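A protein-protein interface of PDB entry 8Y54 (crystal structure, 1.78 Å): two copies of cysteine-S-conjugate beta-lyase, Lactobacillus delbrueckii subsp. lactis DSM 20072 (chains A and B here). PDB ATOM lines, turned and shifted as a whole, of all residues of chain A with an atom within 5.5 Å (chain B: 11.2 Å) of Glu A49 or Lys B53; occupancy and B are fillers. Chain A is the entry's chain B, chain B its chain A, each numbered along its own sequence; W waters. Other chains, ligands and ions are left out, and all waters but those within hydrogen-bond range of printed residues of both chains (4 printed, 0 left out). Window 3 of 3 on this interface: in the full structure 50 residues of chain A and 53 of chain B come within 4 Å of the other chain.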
ATOM      1  N   ILE A  44     -19.334  26.999  -9.798  1.00  0.00           N
ATOM      2  CA  ILE A  44     -20.129  27.467  -8.663  1.00  0.00           C
ATOM      3  C   ILE A  44     -19.238  27.665  -7.447  1.00  0.00           C
ATOM      4  O   ILE A  44     -19.349  28.674  -6.735  1.00  0.00           O
ATOM      5  CB  ILE A  44     -21.286  26.493  -8.353  1.00  0.00           C
ATOM      6  CG1 ILE A  44     -22.213  26.320  -9.551  1.00  0.00           C
ATOM      7  CG2 ILE A  44     -22.060  26.981  -7.137  1.00  0.00           C
ATOM      8  CD1 ILE A  44     -23.128  25.109  -9.411  1.00  0.00           C
ATOM      9  N   MET A  45     -18.316  26.737  -7.213  1.00  0.00           N
ATOM     10  CA  MET A  45     -17.402  26.831  -6.038  1.00  0.00           C
ATOM     11  C   MET A  45     -16.580  28.123  -6.141  1.00  0.00           C
ATOM     12  O   MET A  45     -16.446  28.815  -5.150  1.00  0.00           O
ATOM     13  CB  MET A  45     -16.490  25.596  -5.941  1.00  0.00           C
ATOM     14  CG  MET A  45     -15.545  25.614  -4.768  1.00  0.00           C
ATOM     15  SD  MET A  45     -16.360  25.179  -3.217  1.00  0.00           S
ATOM     16  CE  MET A  45     -17.564  24.005  -3.813  1.00  0.00           C
ATOM     17  N   THR A  46     -16.107  28.437  -7.342  1.00  0.00           N
ATOM     18  CA  THR A  46     -15.375  29.684  -7.537  1.00  0.00           C
ATOM     19  C   THR A  46     -16.198  30.890  -7.105  1.00  0.00           C
ATOM     20  O   THR A  46     -15.680  31.804  -6.455  1.00  0.00           O
ATOM     21  CB  THR A  46     -14.961  29.802  -8.998  1.00  0.00           C
ATOM     22  OG1 THR A  46     -14.025  28.751  -9.282  1.00  0.00           O
ATOM     23  CG2 THR A  46     -14.322  31.176  -9.295  1.00  0.00           C
ATOM     24  N   SER A  47     -17.485  30.904  -7.440  1.00  0.00           N
ATOM     25  CA  SER A  47     -18.309  32.056  -7.101  1.00  0.00           C
ATOM     26  C   SER A  47     -18.513  32.157  -5.600  1.00  0.00           C
ATOM     27  O   SER A  47     -18.572  33.263  -5.045  1.00  0.00           O
ATOM     28  CB  SER A  47     -19.657  31.967  -7.810  1.00  0.00           C
ATOM     29  OG  SER A  47     -20.477  31.026  -7.126  1.00  0.00           O
ATOM     30  N   MET A  48     -18.638  31.010  -4.926  1.00  0.00           N
ATOM     31  CA  MET A  48     -18.827  31.009  -3.482  1.00  0.00           C
ATOM     32  C   MET A  48     -17.580  31.496  -2.770  1.00  0.00           C
ATOM     33  O   MET A  48     -17.661  32.299  -1.837  1.00  0.00           O
ATOM     34  CB  MET A  48     -19.185  29.605  -3.002  1.00  0.00           C
ATOM     35  CG  MET A  48     -20.623  29.195  -3.303  1.00  0.00           C
ATOM     36  SD  MET A  48     -20.861  27.483  -2.828  1.00  0.00           S
ATOM     37  CE  MET A  48     -22.604  27.297  -3.185  1.00  0.00           C
ATOM     38  N   GLU A  49     -16.416  31.026  -3.209  1.00  0.00           N
ATOM     39  CA  GLU A  49     -15.181  31.421  -2.552  1.00  0.00           C
ATOM     40  C   GLU A  49     -14.898  32.899  -2.774  1.00  0.00           C
ATOM     41  O   GLU A  49     -14.350  33.559  -1.888  1.00  0.00           O
ATOM     42  CB  GLU A  49     -14.043  30.524  -3.046  1.00  0.00           C
ATOM     43  CG  GLU A  49     -14.159  29.133  -2.420  1.00  0.00           C
ATOM     44  CD  GLU A  49     -13.251  28.093  -3.039  1.00  0.00           C
ATOM     45  OE1 GLU A  49     -13.093  27.019  -2.420  1.00  0.00           O
ATOM     46  OE2 GLU A  49     -12.707  28.341  -4.136  1.00  0.00           O
ATOM     47  N   GLU A  50     -15.300  33.444  -3.919  1.00  0.00           N
ATOM     48  CA  GLU A  50     -15.130  34.879  -4.154  1.00  0.00           C
ATOM     49  C   GLU A  50     -16.028  35.708  -3.242  1.00  0.00           C
ATOM     50  O   GLU A  50     -15.611  36.755  -2.732  1.00  0.00           O
ATOM     51  CB  GLU A  50     -15.415  35.227  -5.616  1.00  0.00           C
ATOM     52  CG  GLU A  50     -15.218  36.706  -5.936  1.00  0.00           C
ATOM     53  CD  GLU A  50     -13.745  37.091  -6.074  1.00  0.00           C
ATOM     54  OE1 GLU A  50     -13.452  38.022  -6.844  1.00  0.00           O
ATOM     55  OE2 GLU A  50     -12.879  36.462  -5.428  1.00  0.00           O
ATOM     56  N   LYS A  51     -17.271  35.269  -3.039  1.00  0.00           N
ATOM     57  CA  LYS A  51     -18.165  35.999  -2.158  1.00  0.00           C
ATOM     58  C   LYS A  51     -17.650  35.981  -0.724  1.00  0.00           C
ATOM     59  O   LYS A  51     -17.818  36.956   0.019  1.00  0.00           O
ATOM     60  CB  LYS A  51     -19.575  35.395  -2.251  1.00  0.00           C
ATOM     61  CG  LYS A  51     -20.606  36.010  -1.297  1.00  0.00           C
ATOM     62  CD  LYS A  51     -20.723  37.519  -1.473  1.00  0.00           C
ATOM     63  CE  LYS A  51     -21.795  38.140  -0.571  1.00  0.00           C
ATOM     64  NZ  LYS A  51     -23.194  37.729  -0.957  1.00  0.00           N
ATOM     65  N   LEU A  52     -16.997  34.892  -0.324  1.00  0.00           N
ATOM     66  CA  LEU A  52     -16.539  34.788   1.055  1.00  0.00           C
ATOM     67  C   LEU A  52     -15.448  35.798   1.381  1.00  0.00           C
ATOM     68  O   LEU A  52     -15.304  36.173   2.545  1.00  0.00           O
ATOM     69  CB  LEU A  52     -16.038  33.378   1.331  1.00  0.00           C
ATOM     70  CG  LEU A  52     -17.071  32.359   1.787  1.00  0.00           C
ATOM     71  CD1 LEU A  52     -16.388  31.237   2.548  1.00  0.00           C
ATOM     72  CD2 LEU A  52     -18.144  33.032   2.640  1.00  0.00           C
ATOM     73  N   LYS A  53     -14.704  36.268   0.374  1.00  0.00           N
ATOM     74  CA  LYS A  53     -13.672  37.279   0.580  1.00  0.00           C
ATOM     75  C   LYS A  53     -14.214  38.603   1.088  1.00  0.00           C
ATOM     76  O   LYS A  53     -13.451  39.378   1.682  1.00  0.00           O
ATOM     77  CB  LYS A  53     -12.932  37.514  -0.728  1.00  0.00           C
ATOM     78  CG  LYS A  53     -12.242  36.278  -1.143  1.00  0.00           C
ATOM     79  CD  LYS A  53     -11.697  36.392  -2.511  1.00  0.00           C
ATOM     80  CE  LYS A  53     -11.517  37.782  -3.031  1.00  0.00           C
ATOM     81  NZ  LYS A  53     -10.855  37.530  -4.343  1.00  0.00           N
ATOM     82  N   LYS B  13     -15.068  45.307   1.601  1.00  0.00           N
ATOM     83  CA  LYS B  13     -15.537  45.703   0.279  1.00  0.00           C
ATOM     84  C   LYS B  13     -16.640  44.737  -0.141  1.00  0.00           C
ATOM     85  O   LYS B  13     -16.373  43.564  -0.421  1.00  0.00           O
ATOM     86  CB  LYS B  13     -14.383  45.720  -0.716  1.00  0.00           C
ATOM     87  CG  LYS B  13     -13.200  46.541  -0.236  1.00  0.00           C
ATOM     88  CD  LYS B  13     -11.931  45.707  -0.129  1.00  0.00           C
ATOM     89  CE  LYS B  13     -10.742  46.572   0.248  1.00  0.00           C
ATOM     90  NZ  LYS B  13      -9.463  45.932  -0.163  1.00  0.00           N
ATOM     91  N   GLN B  15     -19.954  43.202  -2.332  1.00  0.00           N
ATOM     92  CA  GLN B  15     -20.427  43.094  -3.696  1.00  0.00           C
ATOM     93  C   GLN B  15     -21.576  44.083  -3.887  1.00  0.00           C
ATOM     94  O   GLN B  15     -21.997  44.776  -2.951  1.00  0.00           O
ATOM     95  CB  GLN B  15     -20.814  41.648  -4.000  1.00  0.00           C
ATOM     96  CG  GLN B  15     -19.617  40.689  -3.907  1.00  0.00           C
ATOM     97  CD  GLN B  15     -19.875  39.355  -4.570  1.00  0.00           C
ATOM     98  OE1 GLN B  15     -21.017  39.041  -4.916  1.00  0.00           O
ATOM     99  NE2 GLN B  15     -18.813  38.560  -4.762  1.00  0.00           N
ATOM    100  N   ARG B  39     -14.852  43.585   9.408  1.00  0.00           N
ATOM    101  CA  ARG B  39     -14.770  42.197   8.981  1.00  0.00           C
ATOM    102  C   ARG B  39     -15.155  41.289  10.140  1.00  0.00           C
ATOM    103  O   ARG B  39     -14.982  41.634  11.310  1.00  0.00           O
ATOM    104  CB  ARG B  39     -13.360  41.853   8.486  1.00  0.00           C
ATOM    105  CG  ARG B  39     -12.831  42.766   7.374  1.00  0.00           C
ATOM    106  CD  ARG B  39     -11.306  42.685   7.256  1.00  0.00           C
ATOM    107  NE  ARG B  39     -10.816  41.315   7.414  1.00  0.00           N
ATOM    108  CZ  ARG B  39     -10.642  40.463   6.407  1.00  0.00           C
ATOM    109  NH1 ARG B  39     -10.911  40.841   5.164  1.00  0.00           N
ATOM    110  NH2 ARG B  39     -10.200  39.233   6.639  1.00  0.00           N
ATOM    111  N   MET B  45     -14.808  33.013   9.933  1.00  0.00           N
ATOM    112  CA  MET B  45     -14.404  32.903   8.535  1.00  0.00           C
ATOM    113  C   MET B  45     -13.809  31.533   8.234  1.00  0.00           C
ATOM    114  O   MET B  45     -14.167  30.895   7.237  1.00  0.00           O
ATOM    115  CB  MET B  45     -13.408  34.024   8.210  1.00  0.00           C
ATOM    116  CG  MET B  45     -13.173  34.274   6.757  1.00  0.00           C
ATOM    117  SD  MET B  45     -14.599  35.018   5.951  1.00  0.00           S
ATOM    118  CE  MET B  45     -14.812  33.759   4.708  1.00  0.00           C
ATOM    119  N   THR B  46     -12.907  31.052   9.103  1.00  0.00           N
ATOM    120  CA  THR B  46     -12.286  29.743   8.891  1.00  0.00           C
ATOM    121  C   THR B  46     -13.324  28.627   8.796  1.00  0.00           C
ATOM    122  O   THR B  46     -13.192  27.710   7.974  1.00  0.00           O
ATOM    123  CB  THR B  46     -11.297  29.441  10.014  1.00  0.00           C
ATOM    124  OG1 THR B  46     -10.295  30.469  10.046  1.00  0.00           O
ATOM    125  CG2 THR B  46     -10.624  28.106   9.767  1.00  0.00           C
ATOM    126  N   SER B  47     -14.383  28.697   9.593  1.00  0.00           N
ATOM    127  CA  SER B  47     -15.393  27.613   9.594  1.00  0.00           C
ATOM    128  C   SER B  47     -16.175  27.638   8.279  1.00  0.00           C
ATOM    129  O   SER B  47     -16.539  26.594   7.786  1.00  0.00           O
ATOM    130  CB  SER B  47     -16.312  27.736  10.762  1.00  0.00           C
ATOM    131  OG  SER B  47     -17.122  28.885  10.650  1.00  0.00           O
ATOM    132  N   MET B  48     -16.387  28.832   7.744  1.00  0.00           N
ATOM    133  CA  MET B  48     -17.123  28.959   6.470  1.00  0.00           C
ATOM    134  C   MET B  48     -16.267  28.437   5.308  1.00  0.00           C
ATOM    135  O   MET B  48     -16.790  27.701   4.485  1.00  0.00           O
ATOM    136  CB  MET B  48     -17.553  30.405   6.247  1.00  0.00           C
ATOM    137  CG  MET B  48     -18.595  30.881   7.217  1.00  0.00           C
ATOM    138  SD  MET B  48     -19.074  32.538   6.730  1.00  0.00           S
ATOM    139  CE  MET B  48     -17.482  33.320   6.814  1.00  0.00           C
ATOM    140  N   GLU B  49     -14.989  28.807   5.280  1.00  0.00           N
ATOM    141  CA  GLU B  49     -14.089  28.315   4.212  1.00  0.00           C
ATOM    142  C   GLU B  49     -13.975  26.792   4.347  1.00  0.00           C
ATOM    143  O   GLU B  49     -13.945  26.115   3.332  1.00  0.00           O
ATOM    144  CB  GLU B  49     -12.728  29.012   4.267  1.00  0.00           C
ATOM    145  CG  GLU B  49     -12.774  30.503   4.017  1.00  0.00           C
ATOM    146  CD  GLU B  49     -11.512  31.243   4.428  1.00  0.00           C
ATOM    147  OE1 GLU B  49     -11.400  32.429   4.109  1.00  0.00           O
ATOM    148  OE2 GLU B  49     -10.645  30.628   5.061  1.00  0.00           O
ATOM    149  N   GLU B  50     -13.915  26.298   5.578  1.00  0.00           N
ATOM    150  CA  GLU B  50     -13.825  24.864   5.802  1.00  0.00           C
ATOM    151  C   GLU B  50     -15.070  24.144   5.295  1.00  0.00           C
ATOM    152  O   GLU B  50     -14.982  23.095   4.638  1.00  0.00           O
ATOM    153  CB  GLU B  50     -13.630  24.606   7.289  1.00  0.00           C
ATOM    154  CG  GLU B  50     -13.902  23.190   7.626  1.00  0.00           C
ATOM    155  CD  GLU B  50     -12.789  22.339   7.163  1.00  0.00           C
ATOM    156  OE1 GLU B  50     -12.958  21.105   7.100  1.00  0.00           O
ATOM    157  OE2 GLU B  50     -11.693  22.904   6.916  1.00  0.00           O
ATOM    158  N   LYS B  51     -16.243  24.678   5.627  1.00  0.00           N
ATOM    159  CA  LYS B  51     -17.495  24.069   5.179  1.00  0.00           C
ATOM    160  C   LYS B  51     -17.583  24.016   3.655  1.00  0.00           C
ATOM    161  O   LYS B  51     -18.008  23.001   3.088  1.00  0.00           O
ATOM    162  CB  LYS B  51     -18.678  24.847   5.771  1.00  0.00           C
ATOM    163  CG  LYS B  51     -20.056  24.287   5.395  1.00  0.00           C
ATOM    164  CD  LYS B  51     -20.167  22.810   5.739  1.00  0.00           C
ATOM    165  CE  LYS B  51     -21.523  22.226   5.324  1.00  0.00           C
ATOM    166  NZ  LYS B  51     -22.700  22.804   6.113  1.00  0.00           N
ATOM    167  N   LEU B  52     -17.204  25.100   2.976  1.00  0.00           N
ATOM    168  CA  LEU B  52     -17.276  25.133   1.518  1.00  0.00           C
ATOM    169  C   LEU B  52     -16.481  24.001   0.879  1.00  0.00           C
ATOM    170  O   LEU B  52     -16.851  23.512  -0.191  1.00  0.00           O
ATOM    171  CB  LEU B  52     -16.771  26.474   0.990  1.00  0.00           C
ATOM    172  CG  LEU B  52     -17.664  27.704   1.039  1.00  0.00           C
ATOM    173  CD1 LEU B  52     -17.113  28.749   0.089  1.00  0.00           C
ATOM    174  CD2 LEU B  52     -19.131  27.365   0.710  1.00  0.00           C
ATOM    175  N   LYS B  53     -15.387  23.572   1.509  1.00  0.00           N
ATOM    176  CA  LYS B  53     -14.572  22.522   0.904  1.00  0.00           C
ATOM    177  C   LYS B  53     -15.293  21.178   0.822  1.00  0.00           C
ATOM    178  O   LYS B  53     -14.847  20.306   0.068  1.00  0.00           O
ATOM    179  CB  LYS B  53     -13.255  22.392   1.676  1.00  0.00           C
ATOM    180  CG  LYS B  53     -12.307  23.541   1.377  1.00  0.00           C
ATOM    181  CD  LYS B  53     -11.851  23.477  -0.076  1.00  0.00           C
ATOM    182  CE  LYS B  53     -11.546  24.859  -0.642  1.00  0.00           C
ATOM    183  NZ  LYS B  53     -10.530  25.565   0.186  1.00  0.00           N
ATOM    184  N   VAL B  54     -16.417  21.006   1.512  1.00  0.00           N
ATOM    185  CA  VAL B  54     -17.225  19.762   1.365  1.00  0.00           C
ATOM    186  C   VAL B  54     -17.582  19.653  -0.117  1.00  0.00           C
ATOM    187  O   VAL B  54     -17.624  18.552  -0.633  1.00  0.00           O
ATOM    188  CB  VAL B  54     -18.461  19.776   2.285  1.00  0.00           C
ATOM    189  CG1 VAL B  54     -19.383  18.603   2.007  1.00  0.00           C
ATOM    190  CG2 VAL B  54     -18.065  19.792   3.749  1.00  0.00           C
ATOM    191  N   ALA B  55     -17.784  20.788  -0.794  1.00  0.00           N
ATOM    192  CA  ALA B  55     -18.040  20.863  -2.263  1.00  0.00           C
ATOM    193  C   ALA B  55     -19.349  20.155  -2.619  1.00  0.00           C
ATOM    194  O   ALA B  55     -19.490  19.771  -3.761  1.00  0.00           O
ATOM    195  CB  ALA B  55     -16.846  20.380  -3.030  1.00  0.00           C
ATOM    196  N   ALA B  56     -20.245  20.009  -1.653  1.00  0.00           N
ATOM    197  CA  ALA B  56     -21.579  19.433  -1.902  1.00  0.00           C
ATOM    198  C   ALA B  56     -22.446  19.937  -0.759  1.00  0.00           C
ATOM    199  O   ALA B  56     -21.990  19.881   0.369  1.00  0.00           O
ATOM    200  CB  ALA B  56     -21.576  17.952  -1.986  1.00  0.00           C
ATOM    201  N   PHE B  57     -23.656  20.369  -1.067  1.00  0.00           N
ATOM    202  CA  PHE B  57     -24.449  21.072  -0.068  1.00  0.00           C
ATOM    203  C   PHE B  57     -25.873  20.520  -0.068  1.00  0.00           C
ATOM    204  O   PHE B  57     -26.841  21.197  -0.425  1.00  0.00           O
ATOM    205  CB  PHE B  57     -24.343  22.579  -0.301  1.00  0.00           C
ATOM    206  CG  PHE B  57     -22.901  23.041  -0.315  1.00  0.00           C
ATOM    207  CD1 PHE B  57     -22.161  23.022   0.850  1.00  0.00           C
ATOM    208  CD2 PHE B  57     -22.272  23.379  -1.496  1.00  0.00           C
ATOM    209  CE1 PHE B  57     -20.812  23.369   0.849  1.00  0.00           C
ATOM    210  CE2 PHE B  57     -20.931  23.748  -1.512  1.00  0.00           C
ATOM    211  CZ  PHE B  57     -20.201  23.734  -0.331  1.00  0.00           C
ATOM    212  N   GLY B  58     -25.988  19.272   0.393  1.00  0.00           N
ATOM    213  CA  GLY B  58     -27.273  18.637   0.591  1.00  0.00           C
ATOM    214  C   GLY B  58     -27.922  19.084   1.885  1.00  0.00           C
ATOM    215  O   GLY B  58     -27.510  20.060   2.515  1.00  0.00           O
ATOM    216  N   GLU B  60     -29.280  19.529   5.637  1.00  0.00           N
ATOM    217  CA  GLU B  60     -28.581  19.598   6.907  1.00  0.00           C
ATOM    218  C   GLU B  60     -29.543  19.418   8.059  1.00  0.00           C
ATOM    219  O   GLU B  60     -30.673  19.908   8.016  1.00  0.00           O
ATOM    220  CB  GLU B  60     -27.858  20.921   7.033  1.00  0.00           C
ATOM    221  CG  GLU B  60     -26.786  20.952   6.007  1.00  0.00           C
ATOM    222  CD  GLU B  60     -25.615  21.785   6.393  1.00  0.00           C
ATOM    223  OE1 GLU B  60     -24.868  22.133   5.465  1.00  0.00           O
ATOM    224  OE2 GLU B  60     -25.454  22.083   7.598  1.00  0.00           O
ATOM    225  N   LEU B 270     -26.445  26.205   4.140  1.00  0.00           N
ATOM    226  CA  LEU B 270     -25.105  25.559   4.052  1.00  0.00           C
ATOM    227  C   LEU B 270     -24.039  26.072   5.029  1.00  0.00           C
ATOM    228  O   LEU B 270     -23.058  25.378   5.181  1.00  0.00           O
ATOM    229  CB  LEU B 270     -24.618  25.582   2.596  1.00  0.00           C
ATOM    230  CG  LEU B 270     -24.080  26.891   2.013  1.00  0.00           C
ATOM    231  CD1 LEU B 270     -23.637  26.667   0.581  1.00  0.00           C
ATOM    232  CD2 LEU B 270     -25.092  28.027   2.052  1.00  0.00           C
ATOM    233  N   LEU B 271     -24.211  27.243   5.615  1.00  0.00           N
ATOM    234  CA  LEU B 271     -23.132  27.785   6.486  1.00  0.00           C
ATOM    235  C   LEU B 271     -23.645  28.024   7.904  1.00  0.00           C
ATOM    236  O   LEU B 271     -22.842  28.120   8.794  1.00  0.00           O
ATOM    237  CB  LEU B 271     -22.616  29.089   5.881  1.00  0.00           C
ATOM    238  CG  LEU B 271     -21.758  28.954   4.629  1.00  0.00           C
ATOM    239  CD1 LEU B 271     -21.227  30.307   4.199  1.00  0.00           C
ATOM    240  CD2 LEU B 271     -20.614  27.992   4.864  1.00  0.00           C
ATOM    241  N   PRO B 274     -22.065  25.394  10.936  1.00  0.00           N
ATOM    242  CA  PRO B 274     -20.645  25.521  11.334  1.00  0.00           C
ATOM    243  C   PRO B 274     -20.265  26.940  11.706  1.00  0.00           C
ATOM    244  O   PRO B 274     -19.493  27.140  12.653  1.00  0.00           O
ATOM    245  CB  PRO B 274     -19.872  25.012  10.105  1.00  0.00           C
ATOM    246  CG  PRO B 274     -20.853  25.054   8.969  1.00  0.00           C
ATOM    247  CD  PRO B 274     -22.210  24.904   9.550  1.00  0.00           C
HETATM  248  O   HOH W   1     -23.596  38.913  -3.505  1.00  0.00           O
HETATM  249  O   HOH W   2     -18.841  35.853  -5.876  1.00  0.00           O
HETATM  250  O   HOH W   3     -12.928  27.521   0.892  1.00  0.00           O
HETATM  251  O   HOH W   4     -15.868  39.575  -3.383  1.00  0.00           O
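Water W2 lies within hydrogen-bond range of the backbone carbonyl oxygen of Ser A47, the side-chain amide nitrogen of Gln B15 and the backbone NH of Lys A51.
Water W1 lies within hydrogen-bond range of NZ of Lys A51 (2.8 Å) and OE1 of Gln B15 (2.9 Å).
Water W4 bridges O of Glu A50 and NE2 of Gln B15.
Water W3 lies within hydrogen-bond range of the backbone carbonyl oxygen (O) of Glu B49 (3.0 Å), the side-chain amino group (NZ) of Lys B53 (3.2 Å) and the side-chain carboxylate (OE1) of Glu A49 (3.4 Å).
Met A48 touches Leu B52, and with the chains exchanged Leu A52 touches Met B48.
Glu A49 touches Leu B52, and with the chains exchanged Leu A52 touches Glu B49.
Glu A49 touches Lys B53, but with the chains exchanged Lys A53 does not touch Glu B49 (6.3 Å).
Leu B52 touches its own counterpart, Leu A52.
Of the 12 pairs that touch across the chains among the printed residues, 7 have their exchanged pair printed and touching as well.
Among the printed residues, pairs that only touch across the chains: Met A45 with Ala B55 (3.5 Å), Met A48 with Leu B52 (3.8 Å), Met A48 with Phe B57 (3.96 Å), Met A48 with Leu B270 (3.96 Å), Glu A49 with Leu B52 (3.9 Å), Lys A51 with Gln B15 (3.7 Å), Leu A52 with Met B48 (3.9 Å), Leu A52 with Glu B49 (3.9 Å) and Leu A52 with Leu B52 (3.6 Å).
The side-chain carboxylate (OE1) of Glu A49 is in salt-bridge range of the side-chain amino group (NZ) of Lys B53 (3.9 Å).
The backbone carbonyl oxygen of Leu B52 lies close to the side-chain sulfur of Met A45 (3.5 Å).
The side-chain sulfur (SD) of Met B45 lies close to the backbone carbonyl oxygen (O) of Leu A52 (3.7 Å).
Glu A49 touches just these residues of chain B: Leu B52 (3.9 Å) and Lys B53 (3.2 Å).
Of chain A, only Glu A49 (3.2 Å) comes within 4 Å of Lys B53.
Met A45 touches two residues of chain B.
No residue of chain B comes within 4 Å of Thr A46.
No residue of chain B comes within 4 Å of Ser A47.
No residue of chain B comes within 4 Å of Glu A50.
Leu A52 touches just these residues of chain B: Met B45, Met B48, Glu B49 and Leu B52.
No residue of chain B comes within 4 Å of Lys A53.
Of the printed residues of chain A, Ala B55 touches Met A45.
Printed residues of chain B within 4 Å of Lys A51: Gln B15.
Of the printed residues of chain A, Leu B270 touches Met A48 (3.96 Å).
Of the printed residues of chain A, Leu B52 touches Met A45 (3.5 Å), Met A48 (3.8 Å), Glu A49 (3.9 Å) and Leu A52 (3.6 Å).
The nearest residue of chain A that does not touch Lys B53 is Met A45 (5.1 Å).
The nearest printed residue of chain B that does not touch Met A48 is Gln B15 (7.0 Å).
Of the 10 printed residues of chain A, 5 touch a printed residue of chain B.
Of the 21 printed residues of chain B, 9 touch a printed residue of chain A.
Hydrophobic or aromatic side chains of chain B within 4 Å of the printed part of chain A: Met B45, Met B48, Leu B52, Ala B55, Phe B57 and Leu B270.
Among the printed residues, Asp or Glu carboxylates within 4 Å of a Lys or Arg side-chain nitrogen of the other chain: Glu A49 with Lys B53.
The side-chain amino group (NZ) of Lys B51 is in hydrogen-bond range of the backbone carbonyl oxygen (O) of Leu B270.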
